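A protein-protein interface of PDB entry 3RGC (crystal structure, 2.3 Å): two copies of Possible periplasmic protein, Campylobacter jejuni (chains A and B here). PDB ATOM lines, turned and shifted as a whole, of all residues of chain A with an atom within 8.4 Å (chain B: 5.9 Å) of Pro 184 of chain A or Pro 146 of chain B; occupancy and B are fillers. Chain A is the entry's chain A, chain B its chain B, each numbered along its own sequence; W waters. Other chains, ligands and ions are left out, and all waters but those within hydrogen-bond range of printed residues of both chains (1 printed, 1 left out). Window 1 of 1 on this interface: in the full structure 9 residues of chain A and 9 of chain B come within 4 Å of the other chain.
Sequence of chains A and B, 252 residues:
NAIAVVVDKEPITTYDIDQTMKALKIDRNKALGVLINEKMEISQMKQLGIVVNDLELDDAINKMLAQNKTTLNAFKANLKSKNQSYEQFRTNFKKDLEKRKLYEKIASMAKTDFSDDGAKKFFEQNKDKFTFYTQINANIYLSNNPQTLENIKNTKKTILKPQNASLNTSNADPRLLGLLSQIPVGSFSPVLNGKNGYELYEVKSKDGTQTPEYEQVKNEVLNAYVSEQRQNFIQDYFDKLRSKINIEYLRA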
ATOM      1  N   ASP A 128      -2.966  -4.165  29.188  1.00  0.00           N
ATOM      2  CA  ASP A 128      -3.360  -2.869  28.658  1.00  0.00           C
ATOM      3  C   ASP A 128      -2.169  -1.945  28.407  1.00  0.00           C
ATOM      4  O   ASP A 128      -2.306  -0.872  27.817  1.00  0.00           O
ATOM      5  CB  ASP A 128      -4.377  -2.206  29.585  1.00  0.00           C
ATOM      6  CG  ASP A 128      -3.807  -1.915  30.955  1.00  0.00           C
ATOM      7  OD1 ASP A 128      -2.674  -1.395  31.027  1.00  0.00           O
ATOM      8  OD2 ASP A 128      -4.485  -2.211  31.960  1.00  0.00           O
ATOM      9  N   LYS A 129      -0.991  -2.355  28.844  1.00  0.00           N
ATOM     10  CA  LYS A 129       0.203  -1.563  28.553  1.00  0.00           C
ATOM     11  C   LYS A 129       0.816  -1.874  27.184  1.00  0.00           C
ATOM     12  O   LYS A 129       1.884  -1.347  26.841  1.00  0.00           O
ATOM     13  CB  LYS A 129       1.244  -1.755  29.645  1.00  0.00           C
ATOM     14  CG  LYS A 129       0.748  -1.350  31.000  1.00  0.00           C
ATOM     15  CD  LYS A 129       1.857  -1.395  32.018  1.00  0.00           C
ATOM     16  CE  LYS A 129       1.278  -1.160  33.402  1.00  0.00           C
ATOM     17  NZ  LYS A 129       0.421   0.060  33.408  1.00  0.00           N
ATOM     18  N   PHE A 130       0.142  -2.724  26.409  1.00  0.00           N
ATOM     19  CA  PHE A 130       0.623  -3.106  25.072  1.00  0.00           C
ATOM     20  C   PHE A 130      -0.518  -3.140  24.078  1.00  0.00           C
ATOM     21  O   PHE A 130      -1.629  -3.582  24.385  1.00  0.00           O
ATOM     22  CB  PHE A 130       1.304  -4.475  25.111  1.00  0.00           C
ATOM     23  CG  PHE A 130       2.346  -4.582  26.170  1.00  0.00           C
ATOM     24  CD1 PHE A 130       3.632  -4.147  25.938  1.00  0.00           C
ATOM     25  CD2 PHE A 130       2.020  -5.070  27.423  1.00  0.00           C
ATOM     26  CE1 PHE A 130       4.584  -4.223  26.932  1.00  0.00           C
ATOM     27  CE2 PHE A 130       2.953  -5.153  28.409  1.00  0.00           C
ATOM     28  CZ  PHE A 130       4.240  -4.725  28.169  1.00  0.00           C
ATOM     29  N   THR A 131      -0.248  -2.671  22.872  1.00  0.00           N
ATOM     30  CA  THR A 131      -1.304  -2.588  21.894  1.00  0.00           C
ATOM     31  C   THR A 131      -0.880  -3.279  20.601  1.00  0.00           C
ATOM     32  O   THR A 131       0.257  -3.750  20.481  1.00  0.00           O
ATOM     33  CB  THR A 131      -1.681  -1.130  21.647  1.00  0.00           C
ATOM     34  OG1 THR A 131      -2.740  -1.066  20.684  1.00  0.00           O
ATOM     35  CG2 THR A 131      -0.467  -0.366  21.144  1.00  0.00           C
ATOM     36  N   TYR A 133      -1.768  -2.887  16.209  1.00  0.00           N
ATOM     37  CA  TYR A 133      -2.449  -2.390  15.040  1.00  0.00           C
ATOM     38  C   TYR A 133      -1.995  -3.193  13.845  1.00  0.00           C
ATOM     39  O   TYR A 133      -0.790  -3.367  13.636  1.00  0.00           O
ATOM     40  CB  TYR A 133      -2.094  -0.920  14.830  1.00  0.00           C
ATOM     41  CG  TYR A 133      -2.617  -0.058  15.950  1.00  0.00           C
ATOM     42  CD1 TYR A 133      -3.843   0.589  15.832  1.00  0.00           C
ATOM     43  CD2 TYR A 133      -1.895   0.091  17.145  1.00  0.00           C
ATOM     44  CE1 TYR A 133      -4.340   1.380  16.862  1.00  0.00           C
ATOM     45  CE2 TYR A 133      -2.378   0.872  18.177  1.00  0.00           C
ATOM     46  CZ  TYR A 133      -3.602   1.513  18.027  1.00  0.00           C
ATOM     47  OH  TYR A 133      -4.095   2.291  19.033  1.00  0.00           O
ATOM     48  N   ASN A 137       0.968   3.230   9.032  1.00  0.00           N
ATOM     49  CA  ASN A 137       1.648   4.026   8.020  1.00  0.00           C
ATOM     50  C   ASN A 137       2.867   4.721   8.635  1.00  0.00           C
ATOM     51  O   ASN A 137       2.769   5.373   9.666  1.00  0.00           O
ATOM     52  CB  ASN A 137       0.696   5.016   7.342  1.00  0.00           C
ATOM     53  CG  ASN A 137       1.398   5.866   6.291  1.00  0.00           C
ATOM     54  OD1 ASN A 137       1.267   5.630   5.094  1.00  0.00           O
ATOM     55  ND2 ASN A 137       2.158   6.851   6.740  1.00  0.00           N
ATOM     56  N   LEU A 179       6.568  -4.034  17.367  1.00  0.00           N
ATOM     57  CA  LEU A 179       7.360  -2.869  17.741  1.00  0.00           C
ATOM     58  C   LEU A 179       6.647  -1.550  17.439  1.00  0.00           C
ATOM     59  O   LEU A 179       6.397  -0.740  18.345  1.00  0.00           O
ATOM     60  CB  LEU A 179       8.711  -2.906  17.021  1.00  0.00           C
ATOM     61  CG  LEU A 179       9.737  -1.912  17.596  1.00  0.00           C
ATOM     62  CD1 LEU A 179      11.157  -2.432  17.478  1.00  0.00           C
ATOM     63  CD2 LEU A 179       9.622  -0.537  16.954  1.00  0.00           C
ATOM     64  N   LEU A 180       6.330  -1.329  16.162  1.00  0.00           N
ATOM     65  CA  LEU A 180       5.750  -0.056  15.716  1.00  0.00           C
ATOM     66  C   LEU A 180       4.378   0.217  16.336  1.00  0.00           C
ATOM     67  O   LEU A 180       4.004   1.371  16.532  1.00  0.00           O
ATOM     68  CB  LEU A 180       5.646  -0.032  14.186  1.00  0.00           C
ATOM     69  CG  LEU A 180       6.986  -0.054  13.469  1.00  0.00           C
ATOM     70  CD1 LEU A 180       6.791   0.136  11.982  1.00  0.00           C
ATOM     71  CD2 LEU A 180       7.910   1.032  14.054  1.00  0.00           C
ATOM     72  N   SER A 181       3.622  -0.839  16.635  1.00  0.00           N
ATOM     73  CA  SER A 181       2.314  -0.653  17.253  1.00  0.00           C
ATOM     74  C   SER A 181       2.402   0.136  18.559  1.00  0.00           C
ATOM     75  O   SER A 181       1.443   0.806  18.927  1.00  0.00           O
ATOM     76  CB  SER A 181       1.627  -1.988  17.527  1.00  0.00           C
ATOM     77  OG  SER A 181       1.212  -2.616  16.340  1.00  0.00           O
ATOM     78  N   GLN A 182       3.526   0.030  19.271  1.00  0.00           N
ATOM     79  CA  GLN A 182       3.681   0.732  20.549  1.00  0.00           C
ATOM     80  C   GLN A 182       4.053   2.208  20.380  1.00  0.00           C
ATOM     81  O   GLN A 182       3.837   3.005  21.283  1.00  0.00           O
ATOM     82  CB  GLN A 182       4.745   0.068  21.440  1.00  0.00           C
ATOM     83  CG  GLN A 182       4.684  -1.431  21.513  1.00  0.00           C
ATOM     84  CD  GLN A 182       3.307  -1.985  21.808  1.00  0.00           C
ATOM     85  OE1 GLN A 182       2.579  -1.477  22.658  1.00  0.00           O
ATOM     86  NE2 GLN A 182       2.930  -3.033  21.075  1.00  0.00           N
ATOM     87  N   ILE A 183       4.635   2.571  19.242  1.00  0.00           N
ATOM     88  CA  ILE A 183       5.126   3.937  19.062  1.00  0.00           C
ATOM     89  C   ILE A 183       3.963   4.915  18.833  1.00  0.00           C
ATOM     90  O   ILE A 183       3.095   4.670  18.003  1.00  0.00           O
ATOM     91  CB  ILE A 183       6.159   4.053  17.914  1.00  0.00           C
ATOM     92  CG1 ILE A 183       7.540   3.546  18.341  1.00  0.00           C
ATOM     93  CG2 ILE A 183       6.336   5.509  17.513  1.00  0.00           C
ATOM     94  CD1 ILE A 183       7.613   2.117  18.703  1.00  0.00           C
ATOM     95  N   PRO A 184       3.933   6.015  19.598  1.00  0.00           N
ATOM     96  CA  PRO A 184       2.925   7.079  19.428  1.00  0.00           C
ATOM     97  C   PRO A 184       2.957   7.688  18.026  1.00  0.00           C
ATOM     98  O   PRO A 184       4.026   7.863  17.440  1.00  0.00           O
ATOM     99  CB  PRO A 184       3.352   8.139  20.462  1.00  0.00           C
ATOM    100  CG  PRO A 184       4.110   7.343  21.514  1.00  0.00           C
ATOM    101  CD  PRO A 184       4.791   6.227  20.782  1.00  0.00           C
ATOM    102  N   VAL A 185       1.800   8.009  17.474  1.00  0.00           N
ATOM    103  CA  VAL A 185       1.821   8.697  16.197  1.00  0.00           C
ATOM    104  C   VAL A 185       2.637   9.959  16.407  1.00  0.00           C
ATOM    105  O   VAL A 185       2.465  10.660  17.410  1.00  0.00           O
ATOM    106  CB  VAL A 185       0.412   9.012  15.656  1.00  0.00           C
ATOM    107  CG1 VAL A 185      -0.609   8.042  16.234  1.00  0.00           C
ATOM    108  CG2 VAL A 185       0.029  10.440  15.947  1.00  0.00           C
ATOM    109  N   GLY A 186       3.555  10.212  15.477  1.00  0.00           N
ATOM    110  CA  GLY A 186       4.420  11.378  15.521  1.00  0.00           C
ATOM    111  C   GLY A 186       5.804  11.065  16.050  1.00  0.00           C
ATOM    112  O   GLY A 186       6.748  11.831  15.855  1.00  0.00           O
ATOM    113  N   SER A 187       5.934   9.929  16.719  1.00  0.00           N
ATOM    114  CA  SER A 187       7.205   9.570  17.331  1.00  0.00           C
ATOM    115  C   SER A 187       7.977   8.541  16.520  1.00  0.00           C
ATOM    116  O   SER A 187       7.423   7.891  15.623  1.00  0.00           O
ATOM    117  CB  SER A 187       6.986   9.073  18.750  1.00  0.00           C
ATOM    118  OG  SER A 187       6.376  10.092  19.528  1.00  0.00           O
ATOM    119  N   PHE A 188       9.261   8.418  16.849  1.00  0.00           N
ATOM    120  CA  PHE A 188      10.193   7.541  16.144  1.00  0.00           C
ATOM    121  C   PHE A 188      10.430   6.245  16.887  1.00  0.00           C
ATOM    122  O   PHE A 188      10.383   6.195  18.118  1.00  0.00           O
ATOM    123  CB  PHE A 188      11.551   8.230  15.949  1.00  0.00           C
ATOM    124  CG  PHE A 188      11.545   9.295  14.905  1.00  0.00           C
ATOM    125  CD1 PHE A 188      11.962   9.017  13.615  1.00  0.00           C
ATOM    126  CD2 PHE A 188      11.101  10.579  15.208  1.00  0.00           C
ATOM    127  CE1 PHE A 188      11.944  10.008  12.634  1.00  0.00           C
ATOM    128  CE2 PHE A 188      11.075  11.580  14.239  1.00  0.00           C
ATOM    129  CZ  PHE A 188      11.501  11.295  12.948  1.00  0.00           C
ATOM    130  N   SER A 189      10.694   5.200  16.114  1.00  0.00           N
ATOM    131  CA  SER A 189      11.207   3.961  16.644  1.00  0.00           C
ATOM    132  C   SER A 189      12.678   4.137  17.050  1.00  0.00           C
ATOM    133  O   SER A 189      13.322   5.115  16.687  1.00  0.00           O
ATOM    134  CB  SER A 189      11.146   2.892  15.556  1.00  0.00           C
ATOM    135  OG  SER A 189      12.091   3.173  14.542  1.00  0.00           O
ATOM    136  N   LEU A 200      12.127   4.385  11.732  1.00  0.00           N
ATOM    137  CA  LEU A 200      10.751   4.407  11.296  1.00  0.00           C
ATOM    138  C   LEU A 200      10.055   5.507  12.061  1.00  0.00           C
ATOM    139  O   LEU A 200      10.259   5.673  13.265  1.00  0.00           O
ATOM    140  CB  LEU A 200      10.082   3.015  11.495  1.00  0.00           C
ATOM    141  CG  LEU A 200      10.568   1.955  10.474  1.00  0.00           C
ATOM    142  CD1 LEU A 200      11.394   0.821  11.084  1.00  0.00           C
ATOM    143  CD2 LEU A 200       9.445   1.377   9.611  1.00  0.00           C
ATOM    144  N   TYR A 201       9.242   6.265  11.339  1.00  0.00           N
ATOM    145  CA  TYR A 201       8.567   7.442  11.862  1.00  0.00           C
ATOM    146  C   TYR A 201       7.063   7.216  11.734  1.00  0.00           C
ATOM    147  O   TYR A 201       6.538   7.140  10.631  1.00  0.00           O
ATOM    148  CB  TYR A 201       9.008   8.636  11.017  1.00  0.00           C
ATOM    149  CG  TYR A 201       8.390   9.952  11.374  1.00  0.00           C
ATOM    150  CD1 TYR A 201       7.922  10.198  12.649  1.00  0.00           C
ATOM    151  CD2 TYR A 201       8.280  10.960  10.419  1.00  0.00           C
ATOM    152  CE1 TYR A 201       7.361  11.419  12.966  1.00  0.00           C
ATOM    153  CE2 TYR A 201       7.718  12.161  10.721  1.00  0.00           C
ATOM    154  CZ  TYR A 201       7.259  12.395  11.995  1.00  0.00           C
ATOM    155  OH  TYR A 201       6.693  13.612  12.303  1.00  0.00           O
ATOM    156  N   GLU A 202       6.362   7.098  12.851  1.00  0.00           N
ATOM    157  CA  GLU A 202       4.972   6.658  12.793  1.00  0.00           C
ATOM    158  C   GLU A 202       3.988   7.757  12.473  1.00  0.00           C
ATOM    159  O   GLU A 202       3.875   8.741  13.202  1.00  0.00           O
ATOM    160  CB  GLU A 202       4.541   5.935  14.065  1.00  0.00           C
ATOM    161  CG  GLU A 202       3.051   5.653  14.080  1.00  0.00           C
ATOM    162  CD  GLU A 202       2.650   4.712  15.194  1.00  0.00           C
ATOM    163  N   VAL A 203       3.261   7.569  11.377  1.00  0.00           N
ATOM    164  CA  VAL A 203       2.306   8.559  10.925  1.00  0.00           C
ATOM    165  C   VAL A 203       0.858   8.182  11.244  1.00  0.00           C
ATOM    166  O   VAL A 203       0.053   9.044  11.595  1.00  0.00           O
ATOM    167  CB  VAL A 203       2.425   8.796   9.417  1.00  0.00           C
ATOM    168  CG1 VAL A 203       1.229   9.570   8.935  1.00  0.00           C
ATOM    169  CG2 VAL A 203       3.720   9.533   9.081  1.00  0.00           C
ATOM    170  N   LYS A 204       0.516   6.902  11.115  1.00  0.00           N
ATOM    171  CA  LYS A 204      -0.874   6.494  11.322  1.00  0.00           C
ATOM    172  C   LYS A 204      -0.937   5.057  11.810  1.00  0.00           C
ATOM    173  O   LYS A 204      -0.191   4.192  11.344  1.00  0.00           O
ATOM    174  CB  LYS A 204      -1.732   6.685  10.041  1.00  0.00           C
ATOM    175  N   SER A 205      -1.803   4.834  12.790  1.00  0.00           N
ATOM    176  CA  SER A 205      -2.203   3.509  13.233  1.00  0.00           C
ATOM    177  C   SER A 205      -3.709   3.633  13.391  1.00  0.00           C
ATOM    178  O   SER A 205      -4.233   4.739  13.366  1.00  0.00           O
ATOM    179  CB  SER A 205      -1.587   3.157  14.596  1.00  0.00           C
ATOM    180  OG  SER A 205      -0.252   3.619  14.729  1.00  0.00           O
ATOM    181  N   GLU A 220       8.583  -6.528  23.057  1.00  0.00           N
ATOM    182  CA  GLU A 220       8.186  -5.330  23.798  1.00  0.00           C
ATOM    183  C   GLU A 220       7.912  -5.699  25.240  1.00  0.00           C
ATOM    184  O   GLU A 220       8.346  -5.007  26.154  1.00  0.00           O
ATOM    185  CB  GLU A 220       6.897  -4.722  23.203  1.00  0.00           C
ATOM    186  CG  GLU A 220       6.940  -4.523  21.691  1.00  0.00           C
ATOM    187  CD  GLU A 220       8.269  -3.967  21.241  1.00  0.00           C
ATOM    188  OE1 GLU A 220       8.664  -2.895  21.758  1.00  0.00           O
ATOM    189  OE2 GLU A 220       8.925  -4.614  20.392  1.00  0.00           O
ATOM    190  N   ALA A 224       9.940  -4.637  28.715  1.00  0.00           N
ATOM    191  CA  ALA A 224       9.209  -3.983  29.794  1.00  0.00           C
ATOM    192  C   ALA A 224       9.340  -4.772  31.098  1.00  0.00           C
ATOM    193  O   ALA A 224       9.418  -4.199  32.189  1.00  0.00           O
ATOM    194  CB  ALA A 224       7.753  -3.864  29.421  1.00  0.00           C
ATOM    195  N   SER B 143       8.295   7.235  31.315  1.00  0.00           N
ATOM    196  CA  SER B 143       8.225   5.784  31.283  1.00  0.00           C
ATOM    197  C   SER B 143       9.022   5.196  30.130  1.00  0.00           C
ATOM    198  O   SER B 143       9.197   5.825  29.082  1.00  0.00           O
ATOM    199  CB  SER B 143       6.767   5.320  31.193  1.00  0.00           C
ATOM    200  OG  SER B 143       6.669   3.932  30.890  1.00  0.00           O
ATOM    201  N   ASN B 144       9.505   3.979  30.349  1.00  0.00           N
ATOM    202  CA  ASN B 144      10.076   3.139  29.308  1.00  0.00           C
ATOM    203  C   ASN B 144       8.991   2.668  28.341  1.00  0.00           C
ATOM    204  O   ASN B 144       9.266   2.304  27.195  1.00  0.00           O
ATOM    205  CB  ASN B 144      10.699   1.902  29.959  1.00  0.00           C
ATOM    206  CG  ASN B 144       9.674   1.073  30.723  1.00  0.00           C
ATOM    207  OD1 ASN B 144       9.114   0.110  30.191  1.00  0.00           O
ATOM    208  ND2 ASN B 144       9.414   1.454  31.974  1.00  0.00           N
ATOM    209  N   ASN B 145       7.756   2.670  28.822  1.00  0.00           N
ATOM    210  CA  ASN B 145       6.632   2.131  28.062  1.00  0.00           C
ATOM    211  C   ASN B 145       5.716   3.256  27.600  1.00  0.00           C
ATOM    212  O   ASN B 145       5.106   3.950  28.415  1.00  0.00           O
ATOM    213  CB  ASN B 145       5.862   1.130  28.925  1.00  0.00           C
ATOM    214  CG  ASN B 145       4.776   0.392  28.165  1.00  0.00           C
ATOM    215  OD1 ASN B 145       4.152   0.918  27.245  1.00  0.00           O
ATOM    216  ND2 ASN B 145       4.538  -0.836  28.563  1.00  0.00           N
ATOM    217  N   PRO B 146       5.632   3.444  26.283  1.00  0.00           N
ATOM    218  CA  PRO B 146       4.863   4.552  25.714  1.00  0.00           C
ATOM    219  C   PRO B 146       3.358   4.328  25.882  1.00  0.00           C
ATOM    220  O   PRO B 146       2.614   5.289  26.045  1.00  0.00           O
ATOM    221  CB  PRO B 146       5.284   4.559  24.244  1.00  0.00           C
ATOM    222  CG  PRO B 146       5.759   3.133  23.969  1.00  0.00           C
ATOM    223  CD  PRO B 146       6.276   2.595  25.261  1.00  0.00           C
ATOM    224  N   GLN B 147       2.927   3.072  25.881  1.00  0.00           N
ATOM    225  CA  GLN B 147       1.518   2.756  26.127  1.00  0.00           C
ATOM    226  C   GLN B 147       1.034   3.059  27.554  1.00  0.00           C
ATOM    227  O   GLN B 147      -0.168   3.218  27.772  1.00  0.00           O
ATOM    228  CB  GLN B 147       1.199   1.301  25.775  1.00  0.00           C
ATOM    229  CG  GLN B 147       0.950   1.079  24.300  1.00  0.00           C
ATOM    230  CD  GLN B 147       0.097   2.169  23.699  1.00  0.00           C
ATOM    231  OE1 GLN B 147      -1.056   2.365  24.098  1.00  0.00           O
ATOM    232  NE2 GLN B 147       0.667   2.905  22.742  1.00  0.00           N
ATOM    233  N   THR B 148       1.948   3.119  28.522  1.00  0.00           N
ATOM    234  CA  THR B 148       1.565   3.494  29.887  1.00  0.00           C
ATOM    235  C   THR B 148       1.342   5.012  29.983  1.00  0.00           C
ATOM    236  O   THR B 148       0.529   5.490  30.784  1.00  0.00           O
ATOM    237  CB  THR B 148       2.599   3.037  30.948  1.00  0.00           C
ATOM    238  OG1 THR B 148       3.716   3.933  30.961  1.00  0.00           O
ATOM    239  CG2 THR B 148       3.083   1.639  30.655  1.00  0.00           C
ATOM    240  N   LEU B 149       2.066   5.765  29.165  1.00  0.00           N
ATOM    241  CA  LEU B 149       1.820   7.195  29.060  1.00  0.00           C
ATOM    242  C   LEU B 149       0.582   7.485  28.214  1.00  0.00           C
ATOM    243  O   LEU B 149      -0.137   8.449  28.477  1.00  0.00           O
ATOM    244  CB  LEU B 149       3.046   7.933  28.514  1.00  0.00           C
ATOM    245  CG  LEU B 149       4.325   7.734  29.327  1.00  0.00           C
ATOM    246  CD1 LEU B 149       5.472   8.506  28.715  1.00  0.00           C
ATOM    247  CD2 LEU B 149       4.116   8.130  30.799  1.00  0.00           C
ATOM    248  N   GLU B 150       0.324   6.651  27.206  1.00  0.00           N
ATOM    249  CA  GLU B 150      -0.895   6.788  26.406  1.00  0.00           C
ATOM    250  C   GLU B 150      -2.121   6.617  27.292  1.00  0.00           C
ATOM    251  O   GLU B 150      -3.040   7.428  27.255  1.00  0.00           O
ATOM    252  CB  GLU B 150      -0.936   5.783  25.252  1.00  0.00           C
ATOM    253  CG  GLU B 150      -0.055   6.147  24.065  1.00  0.00           C
ATOM    254  CD  GLU B 150      -0.465   7.455  23.416  1.00  0.00           C
ATOM    255  OE1 GLU B 150      -1.564   7.960  23.733  1.00  0.00           O
ATOM    256  OE2 GLU B 150       0.314   7.983  22.594  1.00  0.00           O
ATOM    257  N   ASN B 151      -2.129   5.553  28.083  1.00  0.00           N
ATOM    258  CA  ASN B 151      -3.195   5.316  29.053  1.00  0.00           C
ATOM    259  C   ASN B 151      -3.420   6.462  30.073  1.00  0.00           C
ATOM    260  O   ASN B 151      -4.395   6.456  30.812  1.00  0.00           O
ATOM    261  CB  ASN B 151      -2.998   3.958  29.739  1.00  0.00           C
ATOM    262  CG  ASN B 151      -2.998   2.812  28.744  1.00  0.00           C
ATOM    263  OD1 ASN B 151      -3.434   2.985  27.611  1.00  0.00           O
ATOM    264  ND2 ASN B 151      -2.516   1.640  29.156  1.00  0.00           N
ATOM    265  N   VAL B 191       2.325  11.783  23.571  1.00  0.00           N
ATOM    266  CA  VAL B 191       3.444  11.042  24.115  1.00  0.00           C
ATOM    267  C   VAL B 191       4.670  11.258  23.228  1.00  0.00           C
ATOM    268  O   VAL B 191       4.633  11.012  22.021  1.00  0.00           O
ATOM    269  CB  VAL B 191       3.134   9.545  24.237  1.00  0.00           C
ATOM    270  CG1 VAL B 191       4.401   8.775  24.637  1.00  0.00           C
ATOM    271  CG2 VAL B 191       1.989   9.307  25.242  1.00  0.00           C
ATOM    272  N   LEU B 192       5.758  11.715  23.838  1.00  0.00           N
ATOM    273  CA  LEU B 192       6.931  12.165  23.100  1.00  0.00           C
ATOM    274  C   LEU B 192       8.153  11.284  23.364  1.00  0.00           C
ATOM    275  O   LEU B 192       8.305  10.754  24.461  1.00  0.00           O
ATOM    276  CB  LEU B 192       7.261  13.605  23.507  1.00  0.00           C
ATOM    277  CG  LEU B 192       6.187  14.668  23.274  1.00  0.00           C
ATOM    278  CD1 LEU B 192       6.755  16.057  23.536  1.00  0.00           C
ATOM    279  CD2 LEU B 192       5.648  14.562  21.850  1.00  0.00           C
ATOM    280  N   TYR B 198      10.150   7.621  27.193  1.00  0.00           N
ATOM    281  CA  TYR B 198       9.058   8.462  26.702  1.00  0.00           C
ATOM    282  C   TYR B 198       8.641   9.480  27.740  1.00  0.00           C
ATOM    283  O   TYR B 198       8.909   9.304  28.932  1.00  0.00           O
ATOM    284  CB  TYR B 198       7.866   7.601  26.245  1.00  0.00           C
ATOM    285  CG  TYR B 198       8.269   6.691  25.120  1.00  0.00           C
ATOM    286  CD1 TYR B 198       8.322   7.161  23.813  1.00  0.00           C
ATOM    287  CD2 TYR B 198       8.645   5.374  25.364  1.00  0.00           C
ATOM    288  CE1 TYR B 198       8.719   6.348  22.774  1.00  0.00           C
ATOM    289  CE2 TYR B 198       9.048   4.543  24.327  1.00  0.00           C
ATOM    290  CZ  TYR B 198       9.079   5.039  23.030  1.00  0.00           C
ATOM    291  OH  TYR B 198       9.478   4.238  21.980  1.00  0.00           O
HETATM  292  O   HOH W   1       8.452  -2.003  32.469  1.00  0.00           O
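The backbone NH of Glu 202 of chain A lies within hydrogen-bond range of the backbone carbonyl oxygen of Ser 187 of chain A, at 3.1 Å.
The side-chain hydroxyl (OG1) of Thr 148 of chain B sits at hydrogen-bond distance from the side-chain hydroxyl (OG) of Ser 143 of chain B (3.0 Å).
The side-chain hydroxyl (OG) of Ser 143 of chain B sits at hydrogen-bond distance from the backbone NH (N) of Asn 145 of chain B (2.7 Å).
O of Thr 131 of chain A sits at hydrogen-bond distance from NE2 of Gln 182 of chain A (2.8 Å).
The backbone carbonyl oxygen (O) of Gln 147 of chain B lies close to the side-chain amide nitrogen (ND2) of Asn 151 of chain B (3.1 Å).
The backbone NH (N) of Gln 147 of chain B sits at hydrogen-bond distance from the side-chain amide oxygen (OD1) of Asn 145 of chain B, 2.8 Å away.
No position is printed for both chains.
Of the printed residues of chain B, Asp 128 of chain A touches Asn 151 (2.9 Å).
Printed residues of chain B within 4 Å of Lys 129 of chain A: Asn 145, Gln 147 and Thr 148.
Of chain B, only Pro 146, Glu 150 and Val 191 come within 4 Å of Pro 184 of chain A.
Of the printed residues of chain B, Ser 187 of chain A touches Val 191 (3.2 Å).
Pro 146 of chain B touches just these residues of chain A: Gln 182 and Pro 184.
The nearest residue of chain B that does not touch Pro 184 of chain A is Tyr 198 of chain B (4.4 Å).
The nearest residue of chain A that does not touch Pro 146 of chain B is Ile 183 of chain A (4.9 Å).
Gln 147 of chain B touches Lys 129 of chain A (CB to O, 2.9 Å).
Lys 129 of chain A touches Thr 148 of chain B (CD to CG2, 3.5 Å).
Phe 130 of chain A touches Asn 145 of chain B (CE1 to ND2, 3.8 Å).
Thr 131 of chain A touches Gln 147 of chain B.
CG of Pro 146 of chain B touches O of Gln 182 of chain A, at 3.3 Å.
CB of Pro 146 of chain B touches CD of Pro 184 of chain A (3.9 Å).
Glu 150 of chain B touches Pro 184 of chain A.
CG1 of Val 191 of chain B touches CG of Pro 184 of chain A, at 3.4 Å.
Hydrophobic or aromatic side chains of chain B within 4 Å of the printed part of chain A: Pro 146 and Val 191.
Among the printed residues, 12 pairs touch across the chains.
Among the printed residues, no Asp or Glu carboxylate lies within 4 Å of a Lys or Arg side-chain nitrogen of the other chain.
The backbone carbonyl oxygen (O) of Lys 129 of chain A is in hydrogen-bond range of the side-chain amide nitrogen (ND2) of Asn 145 of chain B, at 3.2 Å.
The side-chain hydroxyl (OG) of Ser 187 of chain A is in hydrogen-bond range of the backbone carbonyl oxygen (O) of Val 191 of chain B (3.2 Å).
The side-chain amide nitrogen of Gln 147 of chain B sits at hydrogen-bond distance from the backbone carbonyl oxygen of Gln 182 of chain A, at 3.5 Å.
The backbone carbonyl oxygen (O) of Asp 128 of chain A is in hydrogen-bond range of the side-chain amide nitrogen (ND2) of Asn 151 of chain B, 2.9 Å away.
Water W1 lies within hydrogen-bond range of the backbone carbonyl oxygen of Ala 224 of chain A (2.4 Å) and the side-chain amide oxygen of Asn 144 of chain B (3.2 Å).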
